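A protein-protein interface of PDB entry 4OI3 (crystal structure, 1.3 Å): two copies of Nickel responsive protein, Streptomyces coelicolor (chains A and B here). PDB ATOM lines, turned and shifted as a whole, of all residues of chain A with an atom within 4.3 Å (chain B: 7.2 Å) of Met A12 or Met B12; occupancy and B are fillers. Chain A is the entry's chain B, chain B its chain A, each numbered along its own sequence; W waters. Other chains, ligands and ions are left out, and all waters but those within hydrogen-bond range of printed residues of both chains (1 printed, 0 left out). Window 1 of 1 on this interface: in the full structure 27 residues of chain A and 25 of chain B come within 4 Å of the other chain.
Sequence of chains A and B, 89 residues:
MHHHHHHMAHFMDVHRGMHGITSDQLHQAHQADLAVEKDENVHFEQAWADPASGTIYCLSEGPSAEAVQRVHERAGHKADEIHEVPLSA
A ring nitrogen (ND1) of His A83 is in hydrogen-bond range of the side-chain hydroxyl (OH) of Tyr B57 (2.9 Å). OH of Tyr A57 sits at hydrogen-bond distance from ND1 of His B83, at 2.8 Å.
The backbone carbonyl oxygen (O) of His B10 lies within hydrogen-bond range of the backbone NH (N) of Val B85 (2.8 Å). The backbone carbonyl oxygen (O) of His B83 lies within hydrogen-bond range of the backbone NH (N) of Met B12 (2.9 Å). N of Val B14 sits at hydrogen-bond distance from O of Glu B81, at 2.9 Å. The backbone carbonyl oxygen (O) of Gln B46 sits at hydrogen-bond distance from the backbone NH (N) of Leu B59 (2.9 Å). The backbone carbonyl oxygen (O) of Trp B48 is in hydrogen-bond range of the backbone NH (N) of Tyr B57 (2.8 Å). The backbone carbonyl oxygen of His A83 sits at hydrogen-bond distance from the backbone NH of Met A12 (2.9 Å).
CE of Met A12 touches CE3 of Trp B48, at 3.4 Å. CE1 of Tyr B57 touches CG of Met A12, at 3.8 Å. CE of Met B12 touches CE3 of Trp A48 (3.4 Å). Trp A48 touches Trp B48. Leu B59 touches Trp A48. CB of Val B85 touches CB of Trp A48, at 3.8 Å. CG of Met B12 touches CE1 of Tyr A57, 3.8 Å away. Tyr A57 touches Val B14 (OH to CG2, 3.9 Å). Leu A59 touches Trp B48. Trp B48 touches Val A85.
Printed residues of chain B within 4 Å of His A83: Tyr B57 (2.9 Å). Printed residues of chain B within 4 Å of Val A85: Trp B48 (3.8 Å). Met B12 touches just these residues of chain A: Met A12, Trp A48 and Tyr A57. Of the printed residues of chain A, Val B14 touches Tyr A57 (3.9 Å). Printed residues of chain A within 4 Å of His B83: Tyr A57 (2.8 Å). Printed residues of chain A within 4 Å of Val B85: Trp A48. The nearest printed residue of chain B that does not touch Met A12 is Cys B58 (6.4 Å).
Of the 20 printed residues of chain B, 7 touch a printed residue of chain A. Printed residues of chain B that touch a printed residue of chain A: Met B12, Val B14, Trp B48, Tyr B57, Leu B59, His B83 and Val B85. Hydrophobic or aromatic side chains of chain B that line the printed part of chain A: Met B12, Val B14, Trp B48, Tyr B57, Leu B59, His B83 and Val B85. Hydrophobic or aromatic side chains of chain A within 4 Å of the printed part of chain B: Met A12, Trp A48, Tyr A57, Leu A59, His A83 and Val A85.
Met A12 touches its own counterpart, Met B12. Trp A48 touches Leu B59, and with the chains exchanged Leu A59 touches Trp B48. Tyr A57 touches its own counterpart, Tyr B57. Tyr A57 touches His B83, and with the chains exchanged His A83 touches Tyr B57. Positions printed for both chains: 11, 12, 13, 48, 57, 58, 59, 82, 83 and 85. Of the 14 pairs that touch across the chains among the printed residues, 13 have their exchanged pair printed and touching as well.
Water W1 bridges the side-chain hydroxyl (OH) of Tyr A57 (2.8 Å) and the side-chain carboxylate (OE1) of Glu B81 (2.8 Å).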
ATOM      1  N   PHE A  11      -2.601   6.808  14.599  1.00  0.00           N
ATOM      2  CA  PHE A  11      -2.417   7.985  13.740  1.00  0.00           C
ATOM      3  C   PHE A  11      -0.997   8.120  13.224  1.00  0.00           C
ATOM      4  O   PHE A  11      -0.035   7.858  13.947  1.00  0.00           O
ATOM      5  CB  PHE A  11      -2.816   9.273  14.481  1.00  0.00           C
ATOM      6  CG  PHE A  11      -4.260   9.303  14.841  1.00  0.00           C
ATOM      7  CD1 PHE A  11      -4.697   8.783  16.053  1.00  0.00           C
ATOM      8  CD2 PHE A  11      -5.195   9.786  13.939  1.00  0.00           C
ATOM      9  CE1 PHE A  11      -6.044   8.758  16.358  1.00  0.00           C
ATOM     10  CE2 PHE A  11      -6.536   9.764  14.242  1.00  0.00           C
ATOM     11  CZ  PHE A  11      -6.953   9.247  15.447  1.00  0.00           C
ATOM     12  N   MET A  12      -0.885   8.548  11.973  1.00  0.00           N
ATOM     13  CA  MET A  12       0.386   9.002  11.417  1.00  0.00           C
ATOM     14  C   MET A  12       0.241  10.469  11.084  1.00  0.00           C
ATOM     15  O   MET A  12      -0.700  10.854  10.392  1.00  0.00           O
ATOM     16  CB  MET A  12       0.767   8.217  10.161  1.00  0.00           C
ATOM     17  CG  MET A  12       2.135   8.621   9.607  1.00  0.00           C
ATOM     18  SD  MET A  12       3.646   7.974  10.701  1.00  0.00           S
ATOM     19  CE  MET A  12       3.739   6.162  10.001  1.00  0.00           C
ATOM     20  N   ASP A  13       1.153  11.286  11.605  1.00  0.00           N
ATOM     21  CA  ASP A  13       1.137  12.707  11.298  1.00  0.00           C
ATOM     22  C   ASP A  13       2.477  13.157  10.734  1.00  0.00           C
ATOM     23  O   ASP A  13       3.506  12.492  10.917  1.00  0.00           O
ATOM     24  CB  ASP A  13       0.605  13.568  12.468  1.00  0.00           C
ATOM     25  CG  ASP A  13       1.587  13.733  13.610  1.00  0.00           C
ATOM     26  OD1 ASP A  13       2.723  14.194  13.388  1.00  0.00           O
ATOM     27  OD2 ASP A  13       1.187  13.466  14.763  1.00  0.00           O
ATOM     28  N   TRP A  48      10.178   9.618  13.113  1.00  0.00           N
ATOM     29  CA  TRP A  48      11.266   9.474  12.148  1.00  0.00           C
ATOM     30  C   TRP A  48      11.431  10.811  11.446  1.00  0.00           C
ATOM     31  O   TRP A  48      10.432  11.432  11.079  1.00  0.00           O
ATOM     32  CB  TRP A  48      10.933   8.414  11.103  1.00  0.00           C
ATOM     33  CG  TRP A  48      10.600   7.045  11.615  1.00  0.00           C
ATOM     34  CD1 TRP A  48      11.456   5.987  11.768  1.00  0.00           C
ATOM     35  CD2 TRP A  48       9.299   6.574  11.992  1.00  0.00           C
ATOM     36  NE1 TRP A  48      10.763   4.887  12.236  1.00  0.00           N
ATOM     37  CE2 TRP A  48       9.440   5.224  12.382  1.00  0.00           C
ATOM     38  CE3 TRP A  48       8.028   7.172  12.060  1.00  0.00           C
ATOM     39  CZ2 TRP A  48       8.355   4.454  12.812  1.00  0.00           C
ATOM     40  CZ3 TRP A  48       6.952   6.405  12.490  1.00  0.00           C
ATOM     41  CH2 TRP A  48       7.123   5.061  12.855  1.00  0.00           C
ATOM     42  N   TYR A  57       7.826  12.323  10.571  1.00  0.00           N
ATOM     43  CA  TYR A  57       6.694  11.417  10.664  1.00  0.00           C
ATOM     44  C   TYR A  57       6.540  10.999  12.115  1.00  0.00           C
ATOM     45  O   TYR A  57       7.513  10.587  12.750  1.00  0.00           O
ATOM     46  CB  TYR A  57       6.941  10.176   9.811  1.00  0.00           C
ATOM     47  CG  TYR A  57       7.090  10.462   8.333  1.00  0.00           C
ATOM     48  CD1 TYR A  57       8.347  10.675   7.767  1.00  0.00           C
ATOM     49  CD2 TYR A  57       5.972  10.532   7.504  1.00  0.00           C
ATOM     50  CE1 TYR A  57       8.482  10.946   6.408  1.00  0.00           C
ATOM     51  CE2 TYR A  57       6.095  10.801   6.151  1.00  0.00           C
ATOM     52  CZ  TYR A  57       7.350  11.007   5.607  1.00  0.00           C
ATOM     53  OH  TYR A  57       7.457  11.276   4.257  1.00  0.00           O
ATOM     54  N   CYS A  58       5.313  11.099  12.628  1.00  0.00           N
ATOM     55  CA  CYS A  58       5.014  10.704  14.011  1.00  0.00           C
ATOM     56  C   CYS A  58       3.873   9.711  14.063  1.00  0.00           C
ATOM     57  O   CYS A  58       2.777   9.994  13.600  1.00  0.00           O
ATOM     58  CB  CYS A  58       4.621  11.904  14.875  1.00  0.00           C
ATOM     59  SG  CYS A  58       5.918  13.106  15.177  1.00  0.00           S
ATOM     60  N   LEU A  59       4.132   8.552  14.663  1.00  0.00           N
ATOM     61  CA  LEU A  59       3.113   7.516  14.838  1.00  0.00           C
ATOM     62  C   LEU A  59       2.624   7.550  16.280  1.00  0.00           C
ATOM     63  O   LEU A  59       3.442   7.545  17.204  1.00  0.00           O
ATOM     64  CB  LEU A  59       3.693   6.136  14.511  1.00  0.00           C
ATOM     65  CG  LEU A  59       2.763   4.927  14.627  1.00  0.00           C
ATOM     66  CD1 LEU A  59       1.729   4.909  13.507  1.00  0.00           C
ATOM     67  CD2 LEU A  59       3.579   3.646  14.615  1.00  0.00           C
ATOM     68  N   ILE A  82      -2.468  14.960   9.249  1.00  0.00           N
ATOM     69  CA  ILE A  82      -2.680  13.858  10.191  1.00  0.00           C
ATOM     70  C   ILE A  82      -3.714  12.881   9.633  1.00  0.00           C
ATOM     71  O   ILE A  82      -4.765  13.297   9.146  1.00  0.00           O
ATOM     72  CB  ILE A  82      -3.040  14.341  11.624  1.00  0.00           C
ATOM     73  CG1 ILE A  82      -3.260  13.142  12.556  1.00  0.00           C
ATOM     74  CG2 ILE A  82      -4.242  15.292  11.608  1.00  0.00           C
ATOM     75  CD1 ILE A  82      -3.152  13.473  14.019  1.00  0.00           C
ATOM     76  N   HIS A  83      -3.377  11.594   9.679  1.00  0.00           N
ATOM     77  CA  HIS A  83      -4.214  10.531   9.127  1.00  0.00           C
ATOM     78  C   HIS A  83      -4.401   9.432  10.141  1.00  0.00           C
ATOM     79  O   HIS A  83      -3.424   8.944  10.713  1.00  0.00           O
ATOM     80  CB  HIS A  83      -3.534   9.916   7.906  1.00  0.00           C
ATOM     81  CG  HIS A  83      -3.409  10.858   6.756  1.00  0.00           C
ATOM     82  ND1 HIS A  83      -2.202  11.148   6.162  1.00  0.00           N
ATOM     83  CD2 HIS A  83      -4.338  11.603   6.113  1.00  0.00           C
ATOM     84  CE1 HIS A  83      -2.397  12.013   5.182  1.00  0.00           C
ATOM     85  NE2 HIS A  83      -3.682  12.312   5.137  1.00  0.00           N
ATOM     86  N   VAL A  85      -4.646   5.718  10.795  1.00  0.00           N
ATOM     87  CA  VAL A  85      -4.146   4.547  10.074  1.00  0.00           C
ATOM     88  C   VAL A  85      -4.684   3.260  10.720  1.00  0.00           C
ATOM     89  O   VAL A  85      -3.973   2.549  11.430  1.00  0.00           O
ATOM     90  CB  VAL A  85      -2.590   4.551   9.937  1.00  0.00           C
ATOM     91  CG1 VAL A  85      -2.171   5.580   8.893  1.00  0.00           C
ATOM     92  CG2 VAL A  85      -1.891   4.827  11.269  1.00  0.00           C
ATOM     93  N   HIS B  10      17.500   3.881   6.558  1.00  0.00           N
ATOM     94  CA  HIS B  10      16.076   3.741   6.854  1.00  0.00           C
ATOM     95  C   HIS B  10      15.274   4.683   5.980  1.00  0.00           C
ATOM     96  O   HIS B  10      15.687   5.829   5.769  1.00  0.00           O
ATOM     97  CB  HIS B  10      15.826   4.064   8.328  1.00  0.00           C
ATOM     98  CG  HIS B  10      16.775   3.373   9.254  1.00  0.00           C
ATOM     99  ND1 HIS B  10      16.619   2.057   9.634  1.00  0.00           N
ATOM    100  CD2 HIS B  10      17.905   3.809   9.859  1.00  0.00           C
ATOM    101  CE1 HIS B  10      17.607   1.716  10.441  1.00  0.00           C
ATOM    102  NE2 HIS B  10      18.399   2.761  10.597  1.00  0.00           N
ATOM    103  N   PHE B  11      14.129   4.203   5.483  1.00  0.00           N
ATOM    104  CA  PHE B  11      13.287   4.973   4.566  1.00  0.00           C
ATOM    105  C   PHE B  11      11.824   4.951   4.955  1.00  0.00           C
ATOM    106  O   PHE B  11      11.311   3.923   5.414  1.00  0.00           O
ATOM    107  CB  PHE B  11      13.457   4.467   3.129  1.00  0.00           C
ATOM    108  CG  PHE B  11      14.872   4.553   2.651  1.00  0.00           C
ATOM    109  CD1 PHE B  11      15.758   3.503   2.870  1.00  0.00           C
ATOM    110  CD2 PHE B  11      15.342   5.712   2.055  1.00  0.00           C
ATOM    111  CE1 PHE B  11      17.091   3.602   2.484  1.00  0.00           C
ATOM    112  CE2 PHE B  11      16.677   5.815   1.662  1.00  0.00           C
ATOM    113  CZ  PHE B  11      17.545   4.763   1.884  1.00  0.00           C
ATOM    114  N   MET B  12      11.173   6.092   4.754  1.00  0.00           N
ATOM    115  CA  MET B  12       9.723   6.161   4.847  1.00  0.00           C
ATOM    116  C   MET B  12       9.212   6.528   3.468  1.00  0.00           C
ATOM    117  O   MET B  12       9.666   7.509   2.868  1.00  0.00           O
ATOM    118  CB  MET B  12       9.275   7.203   5.873  1.00  0.00           C
ATOM    119  CG  MET B  12       7.764   7.243   6.060  1.00  0.00           C
ATOM    120  SD  MET B  12       7.070   5.699   7.029  1.00  0.00           S
ATOM    121  CE  MET B  12       7.523   6.309   8.829  1.00  0.00           C
ATOM    122  N   ASP B  13       8.286   5.734   2.949  1.00  0.00           N
ATOM    123  CA  ASP B  13       7.696   6.059   1.664  1.00  0.00           C
ATOM    124  C   ASP B  13       6.183   6.173   1.759  1.00  0.00           C
ATOM    125  O   ASP B  13       5.567   5.673   2.706  1.00  0.00           O
ATOM    126  CB  ASP B  13       8.186   5.125   0.537  1.00  0.00           C
ATOM    127  CG  ASP B  13       7.600   3.722   0.591  1.00  0.00           C
ATOM    128  OD1 ASP B  13       6.359   3.575   0.505  1.00  0.00           O
ATOM    129  OD2 ASP B  13       8.396   2.753   0.648  1.00  0.00           O
ATOM    130  N   VAL B  14       5.606   6.867   0.786  1.00  0.00           N
ATOM    131  CA  VAL B  14       4.187   7.208   0.824  1.00  0.00           C
ATOM    132  C   VAL B  14       3.539   6.903  -0.517  1.00  0.00           C
ATOM    133  O   VAL B  14       4.081   7.242  -1.579  1.00  0.00           O
ATOM    134  CB  VAL B  14       3.956   8.709   1.174  1.00  0.00           C
ATOM    135  CG1 VAL B  14       2.474   8.988   1.422  1.00  0.00           C
ATOM    136  CG2 VAL B  14       4.772   9.133   2.386  1.00  0.00           C
ATOM    137  N   GLN B  46       7.287  -2.220   8.294  1.00  0.00           N
ATOM    138  CA  GLN B  46       5.908  -1.937   8.684  1.00  0.00           C
ATOM    139  C   GLN B  46       5.213  -1.140   7.588  1.00  0.00           C
ATOM    140  O   GLN B  46       5.841  -0.322   6.915  1.00  0.00           O
ATOM    141  CB  GLN B  46       5.877  -1.116   9.982  1.00  0.00           C
ATOM    142  CG  GLN B  46       6.385  -1.818  11.241  1.00  0.00           C
ATOM    143  CD  GLN B  46       6.107  -1.026  12.505  1.00  0.00           C
ATOM    144  OE1 GLN B  46       4.964  -0.936  12.951  1.00  0.00           O
ATOM    145  NE2 GLN B  46       7.153  -0.446  13.089  1.00  0.00           N
ATOM    146  N   ALA B  47       3.912  -1.370   7.427  1.00  0.00           N
ATOM    147  CA  ALA B  47       3.059  -0.544   6.583  1.00  0.00           C
ATOM    148  C   ALA B  47       1.841  -0.108   7.386  1.00  0.00           C
ATOM    149  O   ALA B  47       1.309  -0.887   8.181  1.00  0.00           O
ATOM    150  CB  ALA B  47       2.621  -1.310   5.349  1.00  0.00           C
ATOM    151  N   TRP B  48       1.415   1.135   7.180  1.00  0.00           N
ATOM    152  CA  TRP B  48       0.215   1.665   7.820  1.00  0.00           C
ATOM    153  C   TRP B  48      -0.622   2.349   6.751  1.00  0.00           C
ATOM    154  O   TRP B  48      -0.084   3.085   5.922  1.00  0.00           O
ATOM    155  CB  TRP B  48       0.568   2.704   8.876  1.00  0.00           C
ATOM    156  CG  TRP B  48       1.530   2.278   9.951  1.00  0.00           C
ATOM    157  CD1 TRP B  48       1.221   1.743  11.163  1.00  0.00           C
ATOM    158  CD2 TRP B  48       2.958   2.414   9.926  1.00  0.00           C
ATOM    159  NE1 TRP B  48       2.369   1.518  11.892  1.00  0.00           N
ATOM    160  CE2 TRP B  48       3.448   1.921  11.151  1.00  0.00           C
ATOM    161  CE3 TRP B  48       3.871   2.878   8.968  1.00  0.00           C
ATOM    162  CZ2 TRP B  48       4.811   1.901  11.459  1.00  0.00           C
ATOM    163  CZ3 TRP B  48       5.225   2.864   9.276  1.00  0.00           C
ATOM    164  CH2 TRP B  48       5.684   2.371  10.510  1.00  0.00           C
ATOM    165  N   ILE B  56      -0.853   5.456   2.181  1.00  0.00           N
ATOM    166  CA  ILE B  56      -0.120   4.314   2.745  1.00  0.00           C
ATOM    167  C   ILE B  56       1.310   4.735   3.059  1.00  0.00           C
ATOM    168  O   ILE B  56       1.999   5.279   2.201  1.00  0.00           O
ATOM    169  CB  ILE B  56      -0.103   3.079   1.802  1.00  0.00           C
ATOM    170  CG1 ILE B  56      -1.520   2.723   1.343  1.00  0.00           C
ATOM    171  CG2 ILE B  56       0.568   1.889   2.487  1.00  0.00           C
ATOM    172  CD1 ILE B  56      -1.558   1.655   0.275  1.00  0.00           C
ATOM    173  N   TYR B  57       1.740   4.468   4.290  1.00  0.00           N
ATOM    174  CA  TYR B  57       3.093   4.760   4.752  1.00  0.00           C
ATOM    175  C   TYR B  57       3.837   3.448   4.901  1.00  0.00           C
ATOM    176  O   TYR B  57       3.305   2.496   5.477  1.00  0.00           O
ATOM    177  CB  TYR B  57       3.058   5.466   6.107  1.00  0.00           C
ATOM    178  CG  TYR B  57       2.404   6.822   6.052  1.00  0.00           C
ATOM    179  CD1 TYR B  57       1.034   6.970   6.297  1.00  0.00           C
ATOM    180  CD2 TYR B  57       3.143   7.961   5.733  1.00  0.00           C
ATOM    181  CE1 TYR B  57       0.429   8.229   6.239  1.00  0.00           C
ATOM    182  CE2 TYR B  57       2.545   9.213   5.668  1.00  0.00           C
ATOM    183  CZ  TYR B  57       1.193   9.336   5.926  1.00  0.00           C
ATOM    184  OH  TYR B  57       0.618  10.583   5.859  1.00  0.00           O
ATOM    185  N   CYS B  58       5.073   3.397   4.403  1.00  0.00           N
ATOM    186  CA  CYS B  58       5.884   2.170   4.493  1.00  0.00           C
ATOM    187  C   CYS B  58       7.253   2.498   5.038  1.00  0.00           C
ATOM    188  O   CYS B  58       7.957   3.349   4.496  1.00  0.00           O
ATOM    189  CB  CYS B  58       6.082   1.514   3.129  1.00  0.00           C
ATOM    190  SG  CYS B  58       4.645   0.746   2.421  1.00  0.00           S
ATOM    191  N   LEU B  59       7.633   1.800   6.104  1.00  0.00           N
ATOM    192  CA  LEU B  59       8.947   1.953   6.718  1.00  0.00           C
ATOM    193  C   LEU B  59       9.821   0.791   6.273  1.00  0.00           C
ATOM    194  O   LEU B  59       9.422  -0.368   6.414  1.00  0.00           O
ATOM    195  CB  LEU B  59       8.831   1.958   8.244  1.00  0.00           C
ATOM    196  CG  LEU B  59      10.150   2.103   9.017  1.00  0.00           C
ATOM    197  CD1 LEU B  59      10.772   3.479   8.835  1.00  0.00           C
ATOM    198  CD2 LEU B  59       9.895   1.824  10.488  1.00  0.00           C
ATOM    199  N   SER B  60      11.016   1.095   5.765  1.00  0.00           N
ATOM    200  CA  SER B  60      11.930   0.065   5.267  1.00  0.00           C
ATOM    201  C   SER B  60      13.370   0.337   5.691  1.00  0.00           C
ATOM    202  O   SER B  60      13.710   1.444   6.110  1.00  0.00           O
ATOM    203  CB  SER B  60      11.864  -0.048   3.739  1.00  0.00           C
ATOM    204  OG  SER B  60      12.349   1.130   3.112  1.00  0.00           O
ATOM    205  N   VAL B  68      14.820   0.610  -2.728  1.00  0.00           N
ATOM    206  CA  VAL B  68      13.473   0.429  -2.174  1.00  0.00           C
ATOM    207  C   VAL B  68      12.439   0.585  -3.299  1.00  0.00           C
ATOM    208  O   VAL B  68      11.499  -0.211  -3.422  1.00  0.00           O
ATOM    209  CB  VAL B  68      13.211   1.422  -1.025  1.00  0.00           C
ATOM    210  CG1 VAL B  68      11.747   1.367  -0.577  1.00  0.00           C
ATOM    211  CG2 VAL B  68      14.139   1.138   0.152  1.00  0.00           C
ATOM    212  N   ALA B  79       6.278   3.855  -5.007  1.00  0.00           N
ATOM    213  CA  ALA B  79       5.781   4.880  -4.094  1.00  0.00           C
ATOM    214  C   ALA B  79       5.778   6.254  -4.751  1.00  0.00           C
ATOM    215  O   ALA B  79       6.615   6.538  -5.621  1.00  0.00           O
ATOM    216  CB  ALA B  79       6.615   4.907  -2.834  1.00  0.00           C
ATOM    217  N   GLU B  81       6.311   9.073  -3.027  1.00  0.00           N
ATOM    218  CA  GLU B  81       7.345   9.845  -2.329  1.00  0.00           C
ATOM    219  C   GLU B  81       8.182   8.882  -1.513  1.00  0.00           C
ATOM    220  O   GLU B  81       7.644   7.934  -0.949  1.00  0.00           O
ATOM    221  CB  GLU B  81       6.719  10.848  -1.349  1.00  0.00           C
ATOM    222  CG  GLU B  81       5.729  11.849  -1.914  1.00  0.00           C
ATOM    223  CD  GLU B  81       5.013  12.618  -0.816  1.00  0.00           C
ATOM    224  OE1 GLU B  81       5.539  12.680   0.320  1.00  0.00           O
ATOM    225  OE2 GLU B  81       3.922  13.157  -1.086  1.00  0.00           O
ATOM    226  N   ILE B  82       9.490   9.124  -1.431  1.00  0.00           N
ATOM    227  CA  ILE B  82      10.341   8.348  -0.537  1.00  0.00           C
ATOM    228  C   ILE B  82      11.404   9.250   0.083  1.00  0.00           C
ATOM    229  O   ILE B  82      12.030  10.049  -0.613  1.00  0.00           O
ATOM    230  CB  ILE B  82      10.948   7.095  -1.238  1.00  0.00           C
ATOM    231  CG1 ILE B  82      11.819   6.302  -0.264  1.00  0.00           C
ATOM    232  CG2 ILE B  82      11.713   7.474  -2.518  1.00  0.00           C
ATOM    233  CD1 ILE B  82      12.118   4.891  -0.707  1.00  0.00           C
ATOM    234  N   HIS B  83      11.573   9.126   1.399  1.00  0.00           N
ATOM    235  CA  HIS B  83      12.535   9.922   2.151  1.00  0.00           C
ATOM    236  C   HIS B  83      13.413   9.023   2.994  1.00  0.00           C
ATOM    237  O   HIS B  83      12.915   8.113   3.658  1.00  0.00           O
ATOM    238  CB  HIS B  83      11.804  10.877   3.093  1.00  0.00           C
ATOM    239  CG  HIS B  83      10.930  11.869   2.396  1.00  0.00           C
ATOM    240  ND1 HIS B  83       9.652  12.160   2.820  1.00  0.00           N
ATOM    241  CD2 HIS B  83      11.152  12.638   1.304  1.00  0.00           C
ATOM    242  CE1 HIS B  83       9.123  13.069   2.019  1.00  0.00           C
ATOM    243  NE2 HIS B  83      10.010  13.370   1.088  1.00  0.00           N
ATOM    244  N   GLU B  84      14.717   9.284   3.005  1.00  0.00           N
ATOM    245  CA  GLU B  84      15.551   8.642   4.004  1.00  0.00           C
ATOM    246  C   GLU B  84      15.214   9.287   5.336  1.00  0.00           C
ATOM    247  O   GLU B  84      15.025  10.498   5.402  1.00  0.00           O
ATOM    248  CB  GLU B  84      17.045   8.805   3.705  1.00  0.00           C
ATOM    249  CG  GLU B  84      17.887   7.894   4.576  1.00  0.00           C
ATOM    250  CD  GLU B  84      19.378   8.055   4.391  1.00  0.00           C
ATOM    251  OE1 GLU B  84      19.817   8.412   3.277  1.00  0.00           O
ATOM    252  OE2 GLU B  84      20.098   7.790   5.377  1.00  0.00           O
ATOM    253  N   VAL B  85      15.135   8.470   6.381  1.00  0.00           N
ATOM    254  CA  VAL B  85      14.852   8.959   7.724  1.00  0.00           C
ATOM    255  C   VAL B  85      16.003   8.548   8.655  1.00  0.00           C
ATOM    256  O   VAL B  85      15.900   7.584   9.406  1.00  0.00           O
ATOM    257  CB  VAL B  85      13.447   8.503   8.228  1.00  0.00           C
ATOM    258  CG1 VAL B  85      12.352   9.328   7.544  1.00  0.00           C
ATOM    259  CG2 VAL B  85      13.210   6.999   7.994  1.00  0.00           C
HETATM  260  O   HOH W   1       5.429  12.816   3.153  1.00  0.00           O
